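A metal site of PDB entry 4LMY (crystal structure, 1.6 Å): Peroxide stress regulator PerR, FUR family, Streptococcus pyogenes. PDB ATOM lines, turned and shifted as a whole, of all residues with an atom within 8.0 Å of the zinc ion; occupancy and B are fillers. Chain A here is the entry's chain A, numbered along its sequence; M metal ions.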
ATOM      1  N   MET A   1      24.874  34.065 -23.151  1.00  0.00           N
ATOM      2  CA  MET A   1      24.581  33.242 -21.985  1.00  0.00           C
ATOM      3  C   MET A   1      25.848  32.939 -21.203  1.00  0.00           C
ATOM      4  O   MET A   1      26.855  32.519 -21.776  1.00  0.00           O
ATOM      5  CB  MET A   1      23.889  31.947 -22.415  1.00  0.00           C
ATOM      6  CG  MET A   1      22.712  31.542 -21.547  1.00  0.00           C
ATOM      7  SD  MET A   1      21.752  30.214 -22.288  1.00  0.00           S
ATOM      8  CE  MET A   1      21.331  30.942 -23.871  1.00  0.00           C
ATOM      9  N   ASP A   2      25.800  33.156 -19.889  1.00  0.00           N
ATOM     10  CA  ASP A   2      26.968  32.961 -19.032  1.00  0.00           C
ATOM     11  C   ASP A   2      27.379  31.501 -18.935  1.00  0.00           C
ATOM     12  O   ASP A   2      26.578  30.602 -19.147  1.00  0.00           O
ATOM     13  CB  ASP A   2      26.704  33.507 -17.626  1.00  0.00           C
ATOM     14  CG  ASP A   2      26.521  35.007 -17.603  1.00  0.00           C
ATOM     15  OD1 ASP A   2      27.034  35.694 -18.515  1.00  0.00           O
ATOM     16  OD2 ASP A   2      25.851  35.518 -16.669  1.00  0.00           O
ATOM     17  N   ILE A   3      28.649  31.275 -18.604  1.00  0.00           N
ATOM     18  CA  ILE A   3      29.160  29.936 -18.352  1.00  0.00           C
ATOM     19  C   ILE A   3      28.440  29.308 -17.159  1.00  0.00           C
ATOM     20  O   ILE A   3      28.251  29.953 -16.122  1.00  0.00           O
ATOM     21  CB  ILE A   3      30.692  29.942 -18.153  1.00  0.00           C
ATOM     22  CG1 ILE A   3      31.394  30.293 -19.462  1.00  0.00           C
ATOM     23  CG2 ILE A   3      31.181  28.593 -17.644  1.00  0.00           C
ATOM     24  CD1 ILE A   3      32.910  30.264 -19.387  1.00  0.00           C
ATOM     25  N   HIS A   4      28.028  28.061 -17.322  1.00  0.00           N
ATOM     26  CA  HIS A   4      27.206  27.355 -16.346  1.00  0.00           C
ATOM     27  C   HIS A   4      27.335  25.850 -16.573  1.00  0.00           C
ATOM     28  O   HIS A   4      27.931  25.422 -17.558  1.00  0.00           O
ATOM     29  CB  HIS A   4      25.738  27.796 -16.443  1.00  0.00           C
ATOM     30  CG  HIS A   4      25.075  27.416 -17.731  1.00  0.00           C
ATOM     31  ND1 HIS A   4      24.902  28.294 -18.781  1.00  0.00           N
ATOM     32  CD2 HIS A   4      24.522  26.248 -18.136  1.00  0.00           C
ATOM     33  CE1 HIS A   4      24.278  27.688 -19.772  1.00  0.00           C
ATOM     34  NE2 HIS A   4      24.047  26.437 -19.411  1.00  0.00           N
ATOM     35  N   SER A   5      26.760  25.059 -15.670  1.00  0.00           N
ATOM     36  CA  SER A   5      26.777  23.613 -15.802  1.00  0.00           C
ATOM     37  C   SER A   5      25.454  22.994 -15.361  1.00  0.00           C
ATOM     38  O   SER A   5      24.791  23.500 -14.463  1.00  0.00           O
ATOM     39  CB  SER A   5      27.937  23.009 -14.996  1.00  0.00           C
ATOM     40  OG  SER A   5      27.940  21.588 -15.088  1.00  0.00           O
ATOM     41  N   HIS A   6      25.079  21.891 -16.005  1.00  0.00           N
ATOM     42  CA  HIS A   6      23.884  21.146 -15.623  1.00  0.00           C
ATOM     43  C   HIS A   6      24.290  19.832 -14.974  1.00  0.00           C
ATOM     44  O   HIS A   6      23.455  18.957 -14.732  1.00  0.00           O
ATOM     45  CB  HIS A   6      22.987  20.872 -16.827  1.00  0.00           C
ATOM     46  CG  HIS A   6      22.637  22.100 -17.609  1.00  0.00           C
ATOM     47  ND1 HIS A   6      21.539  22.888 -17.314  1.00  0.00           N
ATOM     48  CD2 HIS A   6      23.226  22.669 -18.686  1.00  0.00           C
ATOM     49  CE1 HIS A   6      21.474  23.892 -18.174  1.00  0.00           C
ATOM     50  NE2 HIS A   6      22.491  23.782 -19.020  1.00  0.00           N
ATOM     51  N   GLN A   8      25.751  17.433 -16.251  1.00  0.00           N
ATOM     52  CA  GLN A   8      25.654  16.312 -17.182  1.00  0.00           C
ATOM     53  C   GLN A   8      25.948  16.782 -18.605  1.00  0.00           C
ATOM     54  O   GLN A   8      25.728  17.947 -18.933  1.00  0.00           O
ATOM     55  CB  GLN A   8      24.281  15.647 -17.105  1.00  0.00           C
ATOM     56  CG  GLN A   8      23.118  16.571 -17.430  1.00  0.00           C
ATOM     57  CD  GLN A   8      21.787  15.834 -17.459  1.00  0.00           C
ATOM     58  OE1 GLN A   8      21.708  14.684 -17.882  1.00  0.00           O
ATOM     59  NE2 GLN A   8      20.737  16.511 -17.009  1.00  0.00           N
ATOM     60  N   LEU A  10      25.223  17.309 -22.402  1.00  0.00           N
ATOM     61  CA  LEU A  10      24.000  17.577 -23.138  1.00  0.00           C
ATOM     62  C   LEU A  10      24.372  18.126 -24.507  1.00  0.00           C
ATOM     63  O   LEU A  10      25.152  19.068 -24.600  1.00  0.00           O
ATOM     64  CB  LEU A  10      23.147  18.614 -22.406  1.00  0.00           C
ATOM     65  CG  LEU A  10      22.616  18.308 -21.006  1.00  0.00           C
ATOM     66  CD1 LEU A  10      22.068  19.564 -20.350  1.00  0.00           C
ATOM     67  CD2 LEU A  10      21.545  17.220 -21.069  1.00  0.00           C
ATOM     68  N   ASP A  11      23.844  17.534 -25.573  1.00  0.00           N
ATOM     69  CA  ASP A  11      24.061  18.126 -26.888  1.00  0.00           C
ATOM     70  C   ASP A  11      23.207  19.382 -27.016  1.00  0.00           C
ATOM     71  O   ASP A  11      22.449  19.707 -26.108  1.00  0.00           O
ATOM     72  CB  ASP A  11      23.829  17.138 -28.033  1.00  0.00           C
ATOM     73  CG  ASP A  11      22.393  16.642 -28.132  1.00  0.00           C
ATOM     74  OD1 ASP A  11      22.169  15.671 -28.880  1.00  0.00           O
ATOM     75  OD2 ASP A  11      21.484  17.195 -27.476  1.00  0.00           O
ATOM     76  N   ALA A  12      23.326  20.086 -28.143  1.00  0.00           N
ATOM     77  CA  ALA A  12      22.592  21.327 -28.336  1.00  0.00           C
ATOM     78  C   ALA A  12      21.085  21.168 -28.132  1.00  0.00           C
ATOM     79  O   ALA A  12      20.446  21.997 -27.493  1.00  0.00           O
ATOM     80  CB  ALA A  12      22.885  21.913 -29.715  1.00  0.00           C
ATOM     81  N   GLU A  14      19.357  18.593 -26.451  1.00  0.00           N
ATOM     82  CA  GLU A  14      19.017  18.258 -25.072  1.00  0.00           C
ATOM     83  C   GLU A  14      19.269  19.425 -24.121  1.00  0.00           C
ATOM     84  O   GLU A  14      18.602  19.555 -23.091  1.00  0.00           O
ATOM     85  CB  GLU A  14      19.778  17.007 -24.630  1.00  0.00           C
ATOM     86  CG  GLU A  14      19.417  15.756 -25.427  1.00  0.00           C
ATOM     87  CD  GLU A  14      17.994  15.280 -25.194  1.00  0.00           C
ATOM     88  OE1 GLU A  14      17.340  15.763 -24.243  1.00  0.00           O
ATOM     89  OE2 GLU A  14      17.506  14.431 -25.973  1.00  0.00           O
ATOM     90  N   ASN A  15      20.237  20.270 -24.468  1.00  0.00           N
ATOM     91  CA  ASN A  15      20.529  21.441 -23.660  1.00  0.00           C
ATOM     92  C   ASN A  15      19.378  22.439 -23.702  1.00  0.00           C
ATOM     93  O   ASN A  15      18.951  22.938 -22.657  1.00  0.00           O
ATOM     94  CB  ASN A  15      21.816  22.119 -24.114  1.00  0.00           C
ATOM     95  CG  ASN A  15      22.031  23.454 -23.438  1.00  0.00           C
ATOM     96  OD1 ASN A  15      21.794  24.515 -24.039  1.00  0.00           O
ATOM     97  ND2 ASN A  15      22.447  23.422 -22.181  1.00  0.00           N
ATOM     98  N   VAL A  16      18.873  22.728 -24.902  1.00  0.00           N
ATOM     99  CA  VAL A  16      17.716  23.607 -25.008  1.00  0.00           C
ATOM    100  C   VAL A  16      16.584  22.995 -24.201  1.00  0.00           C
ATOM    101  O   VAL A  16      15.893  23.704 -23.462  1.00  0.00           O
ATOM    102  CB  VAL A  16      17.251  23.795 -26.468  1.00  0.00           C
ATOM    103  CG1 VAL A  16      16.010  24.670 -26.515  1.00  0.00           C
ATOM    104  CG2 VAL A  16      18.361  24.414 -27.297  1.00  0.00           C
ATOM    105  N   GLU A  18      16.746  21.029 -21.560  1.00  0.00           N
ATOM    106  CA  GLU A  18      16.992  21.194 -20.139  1.00  0.00           C
ATOM    107  C   GLU A  18      16.734  22.626 -19.665  1.00  0.00           C
ATOM    108  O   GLU A  18      16.187  22.825 -18.582  1.00  0.00           O
ATOM    109  CB  GLU A  18      18.415  20.754 -19.777  1.00  0.00           C
ATOM    110  CG  GLU A  18      18.742  20.828 -18.296  1.00  0.00           C
ATOM    111  CD  GLU A  18      18.100  19.715 -17.466  1.00  0.00           C
ATOM    112  OE1 GLU A  18      18.552  19.499 -16.323  1.00  0.00           O
ATOM    113  OE2 GLU A  18      17.155  19.052 -17.953  1.00  0.00           O
ATOM    114  N   HIS A  19      17.103  23.604 -20.480  1.00  0.00           N
ATOM    115  CA  HIS A  19      16.921  25.014 -20.112  1.00  0.00           C
ATOM    116  C   HIS A  19      15.453  25.426 -19.943  1.00  0.00           C
ATOM    117  O   HIS A  19      15.114  26.082 -18.954  1.00  0.00           O
ATOM    118  CB  HIS A  19      17.626  25.927 -21.111  1.00  0.00           C
ATOM    119  CG  HIS A  19      19.093  26.088 -20.866  1.00  0.00           C
ATOM    120  ND1 HIS A  19      19.636  27.208 -20.270  1.00  0.00           N
ATOM    121  CD2 HIS A  19      20.143  25.263 -21.121  1.00  0.00           C
ATOM    122  CE1 HIS A  19      20.942  27.075 -20.178  1.00  0.00           C
ATOM    123  NE2 HIS A  19      21.279  25.904 -20.685  1.00  0.00           N
ATOM    124  N   GLU A  22      14.006  23.765 -16.824  1.00  0.00           N
ATOM    125  CA  GLU A  22      14.456  24.491 -15.637  1.00  0.00           C
ATOM    126  C   GLU A  22      13.549  25.687 -15.337  1.00  0.00           C
ATOM    127  O   GLU A  22      13.326  26.023 -14.177  1.00  0.00           O
ATOM    128  CB  GLU A  22      15.894  24.964 -15.814  1.00  0.00           C
ATOM    129  CG  GLU A  22      16.942  23.870 -15.708  1.00  0.00           C
ATOM    130  CD  GLU A  22      18.341  24.369 -15.994  1.00  0.00           C
ATOM    131  OE1 GLU A  22      18.478  25.433 -16.637  1.00  0.00           O
ATOM    132  OE2 GLU A  22      19.310  23.705 -15.576  1.00  0.00           O
ATOM    133  N   PHE A  78      18.165  31.650 -27.160  1.00  0.00           N
ATOM    134  CA  PHE A  78      18.717  30.637 -28.060  1.00  0.00           C
ATOM    135  C   PHE A  78      18.672  31.064 -29.528  1.00  0.00           C
ATOM    136  O   PHE A  78      19.442  30.558 -30.350  1.00  0.00           O
ATOM    137  CB  PHE A  78      18.003  29.293 -27.878  1.00  0.00           C
ATOM    138  CG  PHE A  78      18.298  28.631 -26.564  1.00  0.00           C
ATOM    139  CD1 PHE A  78      17.364  28.643 -25.544  1.00  0.00           C
ATOM    140  CD2 PHE A  78      19.516  27.997 -26.353  1.00  0.00           C
ATOM    141  CE1 PHE A  78      17.641  28.028 -24.335  1.00  0.00           C
ATOM    142  CE2 PHE A  78      19.786  27.381 -25.152  1.00  0.00           C
ATOM    143  CZ  PHE A  78      18.845  27.402 -24.140  1.00  0.00           C
ATOM    144  N   GLY A  96      23.038  28.587 -29.951  1.00  0.00           N
ATOM    145  CA  GLY A  96      23.008  27.673 -28.829  1.00  0.00           C
ATOM    146  C   GLY A  96      24.369  27.422 -28.226  1.00  0.00           C
ATOM    147  O   GLY A  96      25.362  28.068 -28.557  1.00  0.00           O
ATOM    148  N   HIS A  97      24.378  26.475 -27.300  1.00  0.00           N
ATOM    149  CA  HIS A  97      25.609  25.954 -26.740  1.00  0.00           C
ATOM    150  C   HIS A  97      25.289  24.533 -26.350  1.00  0.00           C
ATOM    151  O   HIS A  97      24.143  24.097 -26.425  1.00  0.00           O
ATOM    152  CB  HIS A  97      26.030  26.755 -25.505  1.00  0.00           C
ATOM    153  CG  HIS A  97      25.087  26.622 -24.353  1.00  0.00           C
ATOM    154  ND1 HIS A  97      24.077  27.536 -24.110  1.00  0.00           N
ATOM    155  CD2 HIS A  97      24.997  25.700 -23.372  1.00  0.00           C
ATOM    156  CE1 HIS A  97      23.413  27.179 -23.029  1.00  0.00           C
ATOM    157  NE2 HIS A  97      23.953  26.067 -22.563  1.00  0.00           N
ATOM    158  N   GLN A  98      26.303  23.801 -25.910  1.00  0.00           N
ATOM    159  CA  GLN A  98      26.063  22.483 -25.355  1.00  0.00           C
ATOM    160  C   GLN A  98      27.024  22.246 -24.219  1.00  0.00           C
ATOM    161  O   GLN A  98      27.814  23.130 -23.877  1.00  0.00           O
ATOM    162  CB  GLN A  98      26.223  21.400 -26.431  1.00  0.00           C
ATOM    163  CG  GLN A  98      27.614  21.301 -27.001  1.00  0.00           C
ATOM    164  CD  GLN A  98      27.797  20.038 -27.814  1.00  0.00           C
ATOM    165  OE1 GLN A  98      26.906  19.195 -27.881  1.00  0.00           O
ATOM    166  NE2 GLN A  98      28.962  19.890 -28.416  1.00  0.00           N
ATOM    167  N   HIS A  99      26.953  21.068 -23.613  1.00  0.00           N
ATOM    168  CA  HIS A  99      27.831  20.736 -22.506  1.00  0.00           C
ATOM    169  C   HIS A  99      28.522  19.418 -22.781  1.00  0.00           C
ATOM    170  O   HIS A  99      27.870  18.406 -23.046  1.00  0.00           O
ATOM    171  CB  HIS A  99      27.044  20.725 -21.201  1.00  0.00           C
ATOM    172  CG  HIS A  99      26.369  22.027 -20.896  1.00  0.00           C
ATOM    173  ND1 HIS A  99      26.927  22.982 -20.088  1.00  0.00           N
ATOM    174  CD2 HIS A  99      25.197  22.533 -21.342  1.00  0.00           C
ATOM    175  CE1 HIS A  99      26.123  24.030 -20.022  1.00  0.00           C
ATOM    176  NE2 HIS A  99      25.065  23.786 -20.785  1.00  0.00           N
ATOM    177  N   MET A 114      30.991  24.140 -20.887  1.00  0.00           N
ATOM    178  CA  MET A 114      30.090  24.696 -21.885  1.00  0.00           C
ATOM    179  C   MET A 114      30.779  24.967 -23.198  1.00  0.00           C
ATOM    180  O   MET A 114      31.791  25.676 -23.252  1.00  0.00           O
ATOM    181  CB  MET A 114      29.489  25.993 -21.382  1.00  0.00           C
ATOM    182  CG  MET A 114      28.668  26.746 -22.433  1.00  0.00           C
ATOM    183  SD  MET A 114      27.742  28.027 -21.587  1.00  0.00           S
ATOM    184  CE  MET A 114      27.436  27.121 -20.104  1.00  0.00           C
ATOM    185  N   ASP A 115      30.216  24.424 -24.262  1.00  0.00           N
ATOM    186  CA  ASP A 115      30.794  24.550 -25.584  1.00  0.00           C
ATOM    187  C   ASP A 115      29.876  25.301 -26.548  1.00  0.00           C
ATOM    188  O   ASP A 115      28.670  25.094 -26.551  1.00  0.00           O
ATOM    189  CB  ASP A 115      31.078  23.150 -26.133  1.00  0.00           C
ATOM    190  CG  ASP A 115      31.294  23.157 -27.627  1.00  0.00           C
ATOM    191  OD1 ASP A 115      30.360  22.768 -28.354  1.00  0.00           O
ATOM    192  OD2 ASP A 115      32.396  23.562 -28.052  1.00  0.00           O
HETATM  193 ZN    ZN M   1      23.233  24.927 -20.774  1.00  0.00          ZN
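The zinc ion is bound by a ring nitrogen (NE2) of His 99, a ring nitrogen (NE2) of His 19, a ring nitrogen (NE2) of His 4, the side-chain amide nitrogen (ND2) of Asn 15, a ring nitrogen (NE2) of His 6 and a ring nitrogen (NE2) of His 97.
The backbone NH (N) of His 99 sits at hydrogen-bond distance from the backbone carbonyl oxygen (O) of Leu 10 (2.9 Å). OE2 of Glu 22 lies within hydrogen-bond range of ND1 of His 6. A ring nitrogen (ND1) of His 4 is in hydrogen-bond range of the backbone carbonyl oxygen of Asp 2 (2.9 Å).
Of the 23 residues printed, 6 come within 4 Å of the zinc ion. The nearest printed residue that does not touch the zinc ion is Met 114 (4.8 Å).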
